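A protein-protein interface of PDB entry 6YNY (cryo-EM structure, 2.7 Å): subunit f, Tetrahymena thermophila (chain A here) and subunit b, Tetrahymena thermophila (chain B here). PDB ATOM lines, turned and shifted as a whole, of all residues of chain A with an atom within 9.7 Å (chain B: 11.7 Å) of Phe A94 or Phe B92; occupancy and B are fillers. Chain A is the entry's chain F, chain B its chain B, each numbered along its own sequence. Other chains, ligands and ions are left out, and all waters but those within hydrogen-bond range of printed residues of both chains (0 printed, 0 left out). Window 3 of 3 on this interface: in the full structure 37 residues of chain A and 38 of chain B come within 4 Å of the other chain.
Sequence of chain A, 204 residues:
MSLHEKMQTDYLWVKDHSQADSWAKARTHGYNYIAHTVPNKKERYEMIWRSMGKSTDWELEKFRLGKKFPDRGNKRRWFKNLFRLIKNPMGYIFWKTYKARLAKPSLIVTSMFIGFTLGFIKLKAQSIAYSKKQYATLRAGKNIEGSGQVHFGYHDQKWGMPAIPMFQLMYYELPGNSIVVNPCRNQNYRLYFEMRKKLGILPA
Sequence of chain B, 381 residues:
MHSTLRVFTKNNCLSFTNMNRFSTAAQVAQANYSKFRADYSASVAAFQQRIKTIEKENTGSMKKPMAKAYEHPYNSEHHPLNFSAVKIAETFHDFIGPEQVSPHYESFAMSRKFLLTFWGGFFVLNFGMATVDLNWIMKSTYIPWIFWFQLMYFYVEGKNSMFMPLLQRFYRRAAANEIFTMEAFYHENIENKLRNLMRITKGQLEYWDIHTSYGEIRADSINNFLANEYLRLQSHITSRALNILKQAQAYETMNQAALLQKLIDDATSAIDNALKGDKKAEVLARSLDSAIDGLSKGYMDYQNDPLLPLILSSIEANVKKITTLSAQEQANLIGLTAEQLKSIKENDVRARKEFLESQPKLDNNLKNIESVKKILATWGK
O of Pro B98 lies within hydrogen-bond range of NE1 of Trp A95 (3.4 Å). The side-chain amide nitrogen (ND2) of Asn A88 lies within hydrogen-bond range of the backbone carbonyl oxygen (O) of Phe B95. The backbone carbonyl oxygen (O) of Ile B96 is in hydrogen-bond range of the indole nitrogen (NE1) of Trp A95 (3.5 Å). The backbone carbonyl oxygen (O) of Gly B97 lies within hydrogen-bond range of the indole nitrogen (NE1) of Trp A95 (3.3 Å). The guanidinium group (NH2) of Arg A84 sits at hydrogen-bond distance from the side-chain amide oxygen (OE1) of Gln B100, 2.5 Å away.
Among the printed residues, merely in contact across the chains: Tyr A92 with Gln B100, Gly A91 with Ile B96, Phe A94 with Ile B96, Met A90 with Phe B95, Phe A94 with Phe B92, Trp A95 with Glu B99, Asn A88 with Ile B96 and Gly A91 with Gln B100.
Of the 19 printed residues of chain B, 7 touch a printed residue of chain A. Hydrophobic or aromatic side chains of chain B within 4 Å of the printed part of chain A: Phe B92, Phe B95 and Ile B96. Of the 17 printed residues of chain A, 7 touch a printed residue of chain B. Hydrophobic or aromatic side chains of chain A that line the printed part of chain B: Met A90, Tyr A92, Phe A94 and Trp A95. Among the printed residues, 13 pairs touch across the chains. Among the printed residues, no Asp or Glu carboxylate lies within 4 Å of a Lys or Arg side-chain nitrogen of the other chain.
OG1 of Thr A97 sits at hydrogen-bond distance from O of Phe A94, at 3.3 Å. O of Phe A94 lies within hydrogen-bond range of NH2 of Arg A101, at 2.7 Å. The backbone NH of Gly A91 is in hydrogen-bond range of the side-chain amide oxygen of Asn A88 (3.3 Å).
Phe A94 touches just these residues of chain B: Phe B92 (3.7 Å) and Ile B96 (3.6 Å). Phe B92 touches just one residue of chain A: Phe A94. Of chain B, only Ile B96 and Gln B100 come within 4 Å of Gly A91. No residue of chain B comes within 4 Å of Tyr A98. No residue of chain A comes within 4 Å of Thr B91. Printed residues of chain A within 4 Å of Phe B95: Asn A88 and Met A90. Printed residues of chain A within 4 Å of Ile B96: Asn A88 (3.7 Å), Gly A91 (3.4 Å), Phe A94 (3.6 Å) and Trp A95 (3.5 Å). Of the printed residues of chain A, Gly B97 touches Trp A95. Lys A96 touches none of the printed residues of chain B. The nearest residue of chain B that does not touch Phe A94 is His B93 (5.7 Å).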
ATOM      1  N   ARG A  84      -7.784  -9.321 -11.059  1.00  0.00           N
ATOM      2  CA  ARG A  84      -8.142  -8.744  -9.768  1.00  0.00           C
ATOM      3  C   ARG A  84      -8.477  -9.826  -8.754  1.00  0.00           C
ATOM      4  O   ARG A  84      -8.152  -9.699  -7.569  1.00  0.00           O
ATOM      5  CB  ARG A  84      -9.318  -7.793  -9.933  1.00  0.00           C
ATOM      6  CG  ARG A  84      -8.960  -6.478 -10.554  1.00  0.00           C
ATOM      7  CD  ARG A  84     -10.170  -5.822 -11.151  1.00  0.00           C
ATOM      8  NE  ARG A  84     -11.294  -5.783 -10.228  1.00  0.00           N
ATOM      9  CZ  ARG A  84     -12.522  -5.416 -10.571  1.00  0.00           C
ATOM     10  NH1 ARG A  84     -12.787  -5.059 -11.816  1.00  0.00           N
ATOM     11  NH2 ARG A  84     -13.488  -5.410  -9.670  1.00  0.00           N
ATOM     12  N   LEU A  85      -9.136 -10.892  -9.201  1.00  0.00           N
ATOM     13  CA  LEU A  85      -9.412 -12.021  -8.324  1.00  0.00           C
ATOM     14  C   LEU A  85      -8.125 -12.674  -7.844  1.00  0.00           C
ATOM     15  O   LEU A  85      -8.033 -13.108  -6.691  1.00  0.00           O
ATOM     16  CB  LEU A  85     -10.281 -13.034  -9.063  1.00  0.00           C
ATOM     17  CG  LEU A  85     -10.623 -14.342  -8.358  1.00  0.00           C
ATOM     18  CD1 LEU A  85     -11.479 -14.095  -7.145  1.00  0.00           C
ATOM     19  CD2 LEU A  85     -11.323 -15.273  -9.312  1.00  0.00           C
ATOM     20  N   ASN A  88      -6.267  -9.993  -5.341  1.00  0.00           N
ATOM     21  CA  ASN A  88      -6.882  -9.924  -4.016  1.00  0.00           C
ATOM     22  C   ASN A  88      -8.216 -10.645  -4.060  1.00  0.00           C
ATOM     23  O   ASN A  88      -9.275 -10.028  -4.224  1.00  0.00           O
ATOM     24  CB  ASN A  88      -7.059  -8.479  -3.562  1.00  0.00           C
ATOM     25  CG  ASN A  88      -7.506  -8.375  -2.127  1.00  0.00           C
ATOM     26  OD1 ASN A  88      -7.564  -9.370  -1.409  1.00  0.00           O
ATOM     27  ND2 ASN A  88      -7.818  -7.166  -1.697  1.00  0.00           N
ATOM     28  N   PRO A  89      -8.208 -11.969  -3.906  1.00  0.00           N
ATOM     29  CA  PRO A  89      -9.466 -12.711  -4.049  1.00  0.00           C
ATOM     30  C   PRO A  89     -10.469 -12.415  -2.954  1.00  0.00           C
ATOM     31  O   PRO A  89     -11.676 -12.433  -3.221  1.00  0.00           O
ATOM     32  CB  PRO A  89      -9.006 -14.173  -4.026  1.00  0.00           C
ATOM     33  CG  PRO A  89      -7.746 -14.154  -3.270  1.00  0.00           C
ATOM     34  CD  PRO A  89      -7.082 -12.860  -3.588  1.00  0.00           C
ATOM     35  N   MET A  90     -10.018 -12.144  -1.732  1.00  0.00           N
ATOM     36  CA  MET A  90     -10.959 -11.877  -0.656  1.00  0.00           C
ATOM     37  C   MET A  90     -11.605 -10.507  -0.806  1.00  0.00           C
ATOM     38  O   MET A  90     -12.776 -10.333  -0.455  1.00  0.00           O
ATOM     39  CB  MET A  90     -10.260 -11.995   0.694  1.00  0.00           C
ATOM     40  CG  MET A  90     -11.201 -12.250   1.842  1.00  0.00           C
ATOM     41  SD  MET A  90     -12.029 -13.841   1.697  1.00  0.00           S
ATOM     42  CE  MET A  90     -13.744 -13.334   1.769  1.00  0.00           C
ATOM     43  N   GLY A  91     -10.865  -9.527  -1.325  1.00  0.00           N
ATOM     44  CA  GLY A  91     -11.459  -8.231  -1.598  1.00  0.00           C
ATOM     45  C   GLY A  91     -12.388  -8.245  -2.796  1.00  0.00           C
ATOM     46  O   GLY A  91     -13.421  -7.573  -2.799  1.00  0.00           O
ATOM     47  N   TYR A  92     -12.033  -9.007  -3.830  1.00  0.00           N
ATOM     48  CA  TYR A  92     -12.914  -9.144  -4.981  1.00  0.00           C
ATOM     49  C   TYR A  92     -14.195  -9.872  -4.601  1.00  0.00           C
ATOM     50  O   TYR A  92     -15.283  -9.508  -5.057  1.00  0.00           O
ATOM     51  CB  TYR A  92     -12.176  -9.873  -6.104  1.00  0.00           C
ATOM     52  CG  TYR A  92     -12.965 -10.071  -7.371  1.00  0.00           C
ATOM     53  CD1 TYR A  92     -12.895  -9.153  -8.402  1.00  0.00           C
ATOM     54  CD2 TYR A  92     -13.766 -11.184  -7.544  1.00  0.00           C
ATOM     55  CE1 TYR A  92     -13.607  -9.332  -9.560  1.00  0.00           C
ATOM     56  CE2 TYR A  92     -14.482 -11.369  -8.699  1.00  0.00           C
ATOM     57  CZ  TYR A  92     -14.398 -10.441  -9.705  1.00  0.00           C
ATOM     58  OH  TYR A  92     -15.111 -10.625 -10.863  1.00  0.00           O
ATOM     59  N   ILE A  93     -14.086 -10.897  -3.757  1.00  0.00           N
ATOM     60  CA  ILE A  93     -15.265 -11.636  -3.324  1.00  0.00           C
ATOM     61  C   ILE A  93     -16.108 -10.797  -2.374  1.00  0.00           C
ATOM     62  O   ILE A  93     -17.341 -10.793  -2.456  1.00  0.00           O
ATOM     63  CB  ILE A  93     -14.844 -12.969  -2.682  1.00  0.00           C
ATOM     64  CG1 ILE A  93     -14.284 -13.909  -3.745  1.00  0.00           C
ATOM     65  CG2 ILE A  93     -16.016 -13.601  -1.966  1.00  0.00           C
ATOM     66  CD1 ILE A  93     -13.598 -15.114  -3.192  1.00  0.00           C
ATOM     67  N   PHE A  94     -15.464 -10.078  -1.456  1.00  0.00           N
ATOM     68  CA  PHE A  94     -16.200  -9.288  -0.476  1.00  0.00           C
ATOM     69  C   PHE A  94     -17.100  -8.266  -1.154  1.00  0.00           C
ATOM     70  O   PHE A  94     -18.293  -8.172  -0.849  1.00  0.00           O
ATOM     71  CB  PHE A  94     -15.223  -8.598   0.478  1.00  0.00           C
ATOM     72  CG  PHE A  94     -15.891  -7.774   1.535  1.00  0.00           C
ATOM     73  CD1 PHE A  94     -16.182  -8.316   2.766  1.00  0.00           C
ATOM     74  CD2 PHE A  94     -16.225  -6.457   1.298  1.00  0.00           C
ATOM     75  CE1 PHE A  94     -16.791  -7.567   3.733  1.00  0.00           C
ATOM     76  CE2 PHE A  94     -16.836  -5.708   2.263  1.00  0.00           C
ATOM     77  CZ  PHE A  94     -17.119  -6.261   3.482  1.00  0.00           C
ATOM     78  N   TRP A  95     -16.546  -7.484  -2.080  1.00  0.00           N
ATOM     79  CA  TRP A  95     -17.314  -6.412  -2.696  1.00  0.00           C
ATOM     80  C   TRP A  95     -18.293  -6.927  -3.741  1.00  0.00           C
ATOM     81  O   TRP A  95     -19.343  -6.312  -3.949  1.00  0.00           O
ATOM     82  CB  TRP A  95     -16.366  -5.387  -3.309  1.00  0.00           C
ATOM     83  CG  TRP A  95     -15.613  -4.626  -2.284  1.00  0.00           C
ATOM     84  CD1 TRP A  95     -14.280  -4.684  -2.039  1.00  0.00           C
ATOM     85  CD2 TRP A  95     -16.153  -3.697  -1.344  1.00  0.00           C
ATOM     86  NE1 TRP A  95     -13.951  -3.845  -1.012  1.00  0.00           N
ATOM     87  CE2 TRP A  95     -15.086  -3.225  -0.566  1.00  0.00           C
ATOM     88  CE3 TRP A  95     -17.437  -3.215  -1.089  1.00  0.00           C
ATOM     89  CZ2 TRP A  95     -15.261  -2.296   0.449  1.00  0.00           C
ATOM     90  CZ3 TRP A  95     -17.608  -2.296  -0.084  1.00  0.00           C
ATOM     91  CH2 TRP A  95     -16.527  -1.845   0.674  1.00  0.00           C
ATOM     92  N   LYS A  96     -17.977  -8.037  -4.404  1.00  0.00           N
ATOM     93  CA  LYS A  96     -18.904  -8.622  -5.360  1.00  0.00           C
ATOM     94  C   LYS A  96     -20.087  -9.301  -4.689  1.00  0.00           C
ATOM     95  O   LYS A  96     -21.069  -9.605  -5.370  1.00  0.00           O
ATOM     96  CB  LYS A  96     -18.181  -9.627  -6.252  1.00  0.00           C
ATOM     97  CG  LYS A  96     -17.207  -9.010  -7.229  1.00  0.00           C
ATOM     98  CD  LYS A  96     -17.905  -8.161  -8.255  1.00  0.00           C
ATOM     99  CE  LYS A  96     -16.951  -7.713  -9.329  1.00  0.00           C
ATOM    100  NZ  LYS A  96     -17.591  -6.796 -10.289  1.00  0.00           N
ATOM    101  N   THR A  97     -20.014  -9.549  -3.382  1.00  0.00           N
ATOM    102  CA  THR A  97     -21.087 -10.196  -2.640  1.00  0.00           C
ATOM    103  C   THR A  97     -21.664  -9.304  -1.548  1.00  0.00           C
ATOM    104  O   THR A  97     -22.455  -9.784  -0.730  1.00  0.00           O
ATOM    105  CB  THR A  97     -20.592 -11.505  -2.021  1.00  0.00           C
ATOM    106  OG1 THR A  97     -19.491 -11.239  -1.150  1.00  0.00           O
ATOM    107  CG2 THR A  97     -20.154 -12.474  -3.094  1.00  0.00           C
ATOM    108  N   TYR A  98     -21.299  -8.023  -1.516  1.00  0.00           N
ATOM    109  CA  TYR A  98     -21.811  -7.132  -0.481  1.00  0.00           C
ATOM    110  C   TYR A  98     -23.329  -7.034  -0.543  1.00  0.00           C
ATOM    111  O   TYR A  98     -24.018  -7.247   0.461  1.00  0.00           O
ATOM    112  CB  TYR A  98     -21.177  -5.751  -0.621  1.00  0.00           C
ATOM    113  CG  TYR A  98     -21.623  -4.764   0.429  1.00  0.00           C
ATOM    114  CD1 TYR A  98     -20.898  -4.591   1.593  1.00  0.00           C
ATOM    115  CD2 TYR A  98     -22.767  -4.003   0.255  1.00  0.00           C
ATOM    116  CE1 TYR A  98     -21.299  -3.697   2.551  1.00  0.00           C
ATOM    117  CE2 TYR A  98     -23.175  -3.109   1.205  1.00  0.00           C
ATOM    118  CZ  TYR A  98     -22.438  -2.956   2.354  1.00  0.00           C
ATOM    119  OH  TYR A  98     -22.842  -2.061   3.314  1.00  0.00           O
ATOM    120  N   LYS A  99     -23.871  -6.715  -1.718  1.00  0.00           N
ATOM    121  CA  LYS A  99     -25.313  -6.555  -1.842  1.00  0.00           C
ATOM    122  C   LYS A  99     -26.045  -7.860  -1.571  1.00  0.00           C
ATOM    123  O   LYS A  99     -27.154  -7.848  -1.028  1.00  0.00           O
ATOM    124  CB  LYS A  99     -25.657  -6.023  -3.230  1.00  0.00           C
ATOM    125  CG  LYS A  99     -27.110  -5.597  -3.387  1.00  0.00           C
ATOM    126  CD  LYS A  99     -27.399  -4.993  -4.759  1.00  0.00           C
ATOM    127  CE  LYS A  99     -26.500  -3.806  -5.048  1.00  0.00           C
ATOM    128  NZ  LYS A  99     -26.386  -2.912  -3.862  1.00  0.00           N
ATOM    129  N   ALA A 100     -25.443  -8.991  -1.933  1.00  0.00           N
ATOM    130  CA  ALA A 100     -26.055 -10.278  -1.631  1.00  0.00           C
ATOM    131  C   ALA A 100     -25.957 -10.613  -0.152  1.00  0.00           C
ATOM    132  O   ALA A 100     -26.855 -11.262   0.395  1.00  0.00           O
ATOM    133  CB  ALA A 100     -25.400 -11.378  -2.459  1.00  0.00           C
ATOM    134  N   ARG A 101     -24.886 -10.187   0.509  1.00  0.00           N
ATOM    135  CA  ARG A 101     -24.682 -10.473   1.920  1.00  0.00           C
ATOM    136  C   ARG A 101     -25.384  -9.483   2.835  1.00  0.00           C
ATOM    137  O   ARG A 101     -25.261  -9.602   4.058  1.00  0.00           O
ATOM    138  CB  ARG A 101     -23.188 -10.505   2.228  1.00  0.00           C
ATOM    139  CG  ARG A 101     -22.499 -11.737   1.678  1.00  0.00           C
ATOM    140  CD  ARG A 101     -21.020 -11.773   1.978  1.00  0.00           C
ATOM    141  NE  ARG A 101     -20.316 -10.605   1.471  1.00  0.00           N
ATOM    142  CZ  ARG A 101     -19.977  -9.552   2.203  1.00  0.00           C
ATOM    143  NH1 ARG A 101     -20.265  -9.498   3.492  1.00  0.00           N
ATOM    144  NH2 ARG A 101     -19.343  -8.543   1.640  1.00  0.00           N
ATOM    145  N   LEU A 102     -26.109  -8.512   2.282  1.00  0.00           N
ATOM    146  CA  LEU A 102     -26.955  -7.665   3.112  1.00  0.00           C
ATOM    147  C   LEU A 102     -28.080  -8.474   3.740  1.00  0.00           C
ATOM    148  O   LEU A 102     -28.459  -8.232   4.892  1.00  0.00           O
ATOM    149  CB  LEU A 102     -27.523  -6.516   2.284  1.00  0.00           C
ATOM    150  CG  LEU A 102     -26.536  -5.470   1.784  1.00  0.00           C
ATOM    151  CD1 LEU A 102     -27.234  -4.488   0.871  1.00  0.00           C
ATOM    152  CD2 LEU A 102     -25.888  -4.757   2.943  1.00  0.00           C
ATOM    153  N   HIS B  78       0.055   3.583  14.040  1.00  0.00           N
ATOM    154  CA  HIS B  78      -0.045   2.273  13.411  1.00  0.00           C
ATOM    155  C   HIS B  78      -0.062   1.142  14.426  1.00  0.00           C
ATOM    156  O   HIS B  78      -0.620   0.076  14.146  1.00  0.00           O
ATOM    157  CB  HIS B  78       1.113   2.069  12.436  1.00  0.00           C
ATOM    158  CG  HIS B  78       1.007   0.816  11.630  1.00  0.00           C
ATOM    159  ND1 HIS B  78      -0.103   0.511  10.873  1.00  0.00           N
ATOM    160  CD2 HIS B  78       1.873  -0.210  11.460  1.00  0.00           C
ATOM    161  CE1 HIS B  78       0.084  -0.651  10.274  1.00  0.00           C
ATOM    162  NE2 HIS B  78       1.275  -1.108  10.611  1.00  0.00           N
ATOM    163  N   SER B  84      -9.698  -1.087  20.127  1.00  0.00           N
ATOM    164  CA  SER B  84     -11.053  -0.714  19.756  1.00  0.00           C
ATOM    165  C   SER B  84     -11.333  -1.301  18.382  1.00  0.00           C
ATOM    166  O   SER B  84     -10.411  -1.650  17.639  1.00  0.00           O
ATOM    167  CB  SER B  84     -11.243   0.803  19.736  1.00  0.00           C
ATOM    168  OG  SER B  84     -10.379   1.403  18.786  1.00  0.00           O
ATOM    169  N   ALA B  85     -12.618  -1.405  18.054  1.00  0.00           N
ATOM    170  CA  ALA B  85     -13.018  -1.880  16.737  1.00  0.00           C
ATOM    171  C   ALA B  85     -12.718  -0.874  15.637  1.00  0.00           C
ATOM    172  O   ALA B  85     -12.851  -1.216  14.459  1.00  0.00           O
ATOM    173  CB  ALA B  85     -14.505  -2.218  16.737  1.00  0.00           C
ATOM    174  N   VAL B  86     -12.311   0.343  15.991  1.00  0.00           N
ATOM    175  CA  VAL B  86     -12.033   1.361  14.985  1.00  0.00           C
ATOM    176  C   VAL B  86     -10.741   1.043  14.244  1.00  0.00           C
ATOM    177  O   VAL B  86     -10.676   1.130  13.013  1.00  0.00           O
ATOM    178  CB  VAL B  86     -11.987   2.751  15.640  1.00  0.00           C
ATOM    179  CG1 VAL B  86     -11.714   3.820  14.610  1.00  0.00           C
ATOM    180  CG2 VAL B  86     -13.289   3.027  16.352  1.00  0.00           C
ATOM    181  N   LYS B  87      -9.690   0.675  14.977  1.00  0.00           N
ATOM    182  CA  LYS B  87      -8.432   0.344  14.321  1.00  0.00           C
ATOM    183  C   LYS B  87      -8.539  -0.969  13.561  1.00  0.00           C
ATOM    184  O   LYS B  87      -7.943  -1.125  12.491  1.00  0.00           O
ATOM    185  CB  LYS B  87      -7.302   0.278  15.345  1.00  0.00           C
ATOM    186  CG  LYS B  87      -5.929   0.065  14.741  1.00  0.00           C
ATOM    187  CD  LYS B  87      -5.462   1.282  13.984  1.00  0.00           C
ATOM    188  CE  LYS B  87      -4.162   1.027  13.262  1.00  0.00           C
ATOM    189  NZ  LYS B  87      -3.691   2.252  12.576  1.00  0.00           N
ATOM    190  N   ILE B  88      -9.293  -1.927  14.100  1.00  0.00           N
ATOM    191  CA  ILE B  88      -9.524  -3.178  13.389  1.00  0.00           C
ATOM    192  C   ILE B  88     -10.249  -2.915  12.078  1.00  0.00           C
ATOM    193  O   ILE B  88      -9.977  -3.558  11.059  1.00  0.00           O
ATOM    194  CB  ILE B  88     -10.306  -4.157  14.284  1.00  0.00           C
ATOM    195  CG1 ILE B  88      -9.525  -4.443  15.562  1.00  0.00           C
ATOM    196  CG2 ILE B  88     -10.588  -5.444  13.550  1.00  0.00           C
ATOM    197  CD1 ILE B  88     -10.294  -5.239  16.574  1.00  0.00           C
ATOM    198  N   ALA B  89     -11.183  -1.965  12.084  1.00  0.00           N
ATOM    199  CA  ALA B  89     -11.881  -1.608  10.857  1.00  0.00           C
ATOM    200  C   ALA B  89     -10.938  -0.961   9.856  1.00  0.00           C
ATOM    201  O   ALA B  89     -11.055  -1.186   8.647  1.00  0.00           O
ATOM    202  CB  ALA B  89     -13.043  -0.677  11.176  1.00  0.00           C
ATOM    203  N   GLU B  90      -9.999  -0.150  10.341  1.00  0.00           N
ATOM    204  CA  GLU B  90      -9.025   0.469   9.453  1.00  0.00           C
ATOM    205  C   GLU B  90      -8.154  -0.581   8.781  1.00  0.00           C
ATOM    206  O   GLU B  90      -7.865  -0.485   7.583  1.00  0.00           O
ATOM    207  CB  GLU B  90      -8.172   1.462  10.237  1.00  0.00           C
ATOM    208  CG  GLU B  90      -7.326   2.372   9.382  1.00  0.00           C
ATOM    209  CD  GLU B  90      -6.296   3.139  10.186  1.00  0.00           C
ATOM    210  OE1 GLU B  90      -5.302   2.525  10.621  1.00  0.00           O
ATOM    211  OE2 GLU B  90      -6.478   4.357  10.383  1.00  0.00           O
ATOM    212  N   THR B  91      -7.727  -1.596   9.536  1.00  0.00           N
ATOM    213  CA  THR B  91      -6.911  -2.654   8.955  1.00  0.00           C
ATOM    214  C   THR B  91      -7.733  -3.569   8.064  1.00  0.00           C
ATOM    215  O   THR B  91      -7.213  -4.110   7.085  1.00  0.00           O
ATOM    216  CB  THR B  91      -6.240  -3.474  10.054  1.00  0.00           C
ATOM    217  OG1 THR B  91      -7.235  -4.123  10.849  1.00  0.00           O
ATOM    218  CG2 THR B  91      -5.401  -2.596  10.932  1.00  0.00           C
ATOM    219  N   PHE B  92      -9.011  -3.757   8.388  1.00  0.00           N
ATOM    220  CA  PHE B  92      -9.859  -4.616   7.574  1.00  0.00           C
ATOM    221  C   PHE B  92     -10.061  -4.033   6.185  1.00  0.00           C
ATOM    222  O   PHE B  92      -9.983  -4.755   5.186  1.00  0.00           O
ATOM    223  CB  PHE B  92     -11.199  -4.826   8.272  1.00  0.00           C
ATOM    224  CG  PHE B  92     -12.173  -5.637   7.483  1.00  0.00           C
ATOM    225  CD1 PHE B  92     -13.269  -5.045   6.899  1.00  0.00           C
ATOM    226  CD2 PHE B  92     -11.992  -6.993   7.322  1.00  0.00           C
ATOM    227  CE1 PHE B  92     -14.161  -5.786   6.178  1.00  0.00           C
ATOM    228  CE2 PHE B  92     -12.884  -7.736   6.600  1.00  0.00           C
ATOM    229  CZ  PHE B  92     -13.969  -7.130   6.026  1.00  0.00           C
ATOM    230  N   HIS B  93     -10.314  -2.729   6.099  1.00  0.00           N
ATOM    231  CA  HIS B  93     -10.551  -2.107   4.804  1.00  0.00           C
ATOM    232  C   HIS B  93      -9.267  -1.930   4.009  1.00  0.00           C
ATOM    233  O   HIS B  93      -9.308  -1.919   2.776  1.00  0.00           O
ATOM    234  CB  HIS B  93     -11.264  -0.771   4.985  1.00  0.00           C
ATOM    235  CG  HIS B  93     -12.734  -0.910   5.222  1.00  0.00           C
ATOM    236  ND1 HIS B  93     -13.275  -1.045   6.480  1.00  0.00           N
ATOM    237  CD2 HIS B  93     -13.774  -0.958   4.358  1.00  0.00           C
ATOM    238  CE1 HIS B  93     -14.586  -1.159   6.382  1.00  0.00           C
ATOM    239  NE2 HIS B  93     -14.915  -1.111   5.105  1.00  0.00           N
ATOM    240  N   ASP B  94      -8.126  -1.795   4.682  1.00  0.00           N
ATOM    241  CA  ASP B  94      -6.859  -1.857   3.968  1.00  0.00           C
ATOM    242  C   ASP B  94      -6.668  -3.219   3.319  1.00  0.00           C
ATOM    243  O   ASP B  94      -6.039  -3.323   2.261  1.00  0.00           O
ATOM    244  CB  ASP B  94      -5.700  -1.565   4.915  1.00  0.00           C
ATOM    245  CG  ASP B  94      -5.776  -0.183   5.530  1.00  0.00           C
ATOM    246  OD1 ASP B  94      -6.694   0.584   5.170  1.00  0.00           O
ATOM    247  OD2 ASP B  94      -4.916   0.137   6.376  1.00  0.00           O
ATOM    248  N   PHE B  95      -7.211  -4.268   3.934  1.00  0.00           N
ATOM    249  CA  PHE B  95      -7.052  -5.623   3.422  1.00  0.00           C
ATOM    250  C   PHE B  95      -7.984  -5.896   2.247  1.00  0.00           C
ATOM    251  O   PHE B  95      -7.532  -6.264   1.159  1.00  0.00           O
ATOM    252  CB  PHE B  95      -7.275  -6.620   4.559  1.00  0.00           C
ATOM    253  CG  PHE B  95      -7.571  -8.010   4.104  1.00  0.00           C
ATOM    254  CD1 PHE B  95      -8.694  -8.667   4.559  1.00  0.00           C
ATOM    255  CD2 PHE B  95      -6.736  -8.661   3.220  1.00  0.00           C
ATOM    256  CE1 PHE B  95      -8.976  -9.942   4.149  1.00  0.00           C
ATOM    257  CE2 PHE B  95      -7.015  -9.938   2.805  1.00  0.00           C
ATOM    258  CZ  PHE B  95      -8.137 -10.579   3.269  1.00  0.00           C
ATOM    259  N   ILE B  96      -9.294  -5.726   2.445  1.00  0.00           N
ATOM    260  CA  ILE B  96     -10.233  -5.930   1.351  1.00  0.00           C
ATOM    261  C   ILE B  96     -10.137  -4.840   0.302  1.00  0.00           C
ATOM    262  O   ILE B  96     -10.702  -4.984  -0.787  1.00  0.00           O
ATOM    263  CB  ILE B  96     -11.679  -6.024   1.875  1.00  0.00           C
ATOM    264  CG1 ILE B  96     -12.073  -4.740   2.604  1.00  0.00           C
ATOM    265  CG2 ILE B  96     -11.818  -7.214   2.790  1.00  0.00           C
ATOM    266  CD1 ILE B  96     -13.507  -4.677   2.982  1.00  0.00           C
ATOM    267  N   GLY B  97      -9.436  -3.755   0.603  1.00  0.00           N
ATOM    268  CA  GLY B  97      -9.205  -2.707  -0.352  1.00  0.00           C
ATOM    269  C   GLY B  97     -10.411  -1.821  -0.541  1.00  0.00           C
ATOM    270  O   GLY B  97     -11.463  -2.016   0.074  1.00  0.00           O
ATOM    271  N   PRO B  98     -10.277  -0.819  -1.399  1.00  0.00           N
ATOM    272  CA  PRO B  98     -11.397   0.084  -1.656  1.00  0.00           C
ATOM    273  C   PRO B  98     -12.522  -0.613  -2.396  1.00  0.00           C
ATOM    274  O   PRO B  98     -12.349  -1.659  -3.023  1.00  0.00           O
ATOM    275  CB  PRO B  98     -10.773   1.189  -2.510  1.00  0.00           C
ATOM    276  CG  PRO B  98      -9.598   0.557  -3.141  1.00  0.00           C
ATOM    277  CD  PRO B  98      -9.079  -0.438  -2.161  1.00  0.00           C
ATOM    278  N   GLU B  99     -13.697  -0.009  -2.302  1.00  0.00           N
ATOM    279  CA  GLU B  99     -14.864  -0.490  -3.022  1.00  0.00           C
ATOM    280  C   GLU B  99     -14.546  -0.607  -4.502  1.00  0.00           C
ATOM    281  O   GLU B  99     -14.192   0.380  -5.151  1.00  0.00           O
ATOM    282  CB  GLU B  99     -16.026   0.472  -2.789  1.00  0.00           C
ATOM    283  CG  GLU B  99     -17.345   0.036  -3.364  1.00  0.00           C
ATOM    284  CD  GLU B  99     -18.444   1.042  -3.095  1.00  0.00           C
ATOM    285  OE1 GLU B  99     -18.159   2.072  -2.450  1.00  0.00           O
ATOM    286  OE2 GLU B  99     -19.590   0.807  -3.527  1.00  0.00           O
ATOM    287  N   GLN B 100     -14.656  -1.822  -5.033  1.00  0.00           N
ATOM    288  CA  GLN B 100     -14.327  -2.079  -6.433  1.00  0.00           C
ATOM    289  C   GLN B 100     -15.444  -1.515  -7.302  1.00  0.00           C
ATOM    290  O   GLN B 100     -16.378  -2.206  -7.712  1.00  0.00           O
ATOM    291  CB  GLN B 100     -14.121  -3.565  -6.676  1.00  0.00           C
ATOM    292  CG  GLN B 100     -13.031  -4.155  -5.822  1.00  0.00           C
ATOM    293  CD  GLN B 100     -12.485  -5.445  -6.370  1.00  0.00           C
ATOM    294  OE1 GLN B 100     -13.008  -5.999  -7.332  1.00  0.00           O
ATOM    295  NE2 GLN B 100     -11.419  -5.928  -5.761  1.00  0.00           N
ATOM    296  N   VAL B 101     -15.334  -0.224  -7.580  1.00  0.00           N
ATOM    297  CA  VAL B 101     -16.331   0.480  -8.373  1.00  0.00           C
ATOM    298  C   VAL B 101     -16.161   0.103  -9.835  1.00  0.00           C
ATOM    299  O   VAL B 101     -15.064   0.206 -10.395  1.00  0.00           O
ATOM    300  CB  VAL B 101     -16.206   1.997  -8.170  1.00  0.00           C
ATOM    301  CG1 VAL B 101     -17.172   2.733  -9.060  1.00  0.00           C
ATOM    302  CG2 VAL B 101     -16.449   2.350  -6.724  1.00  0.00           C
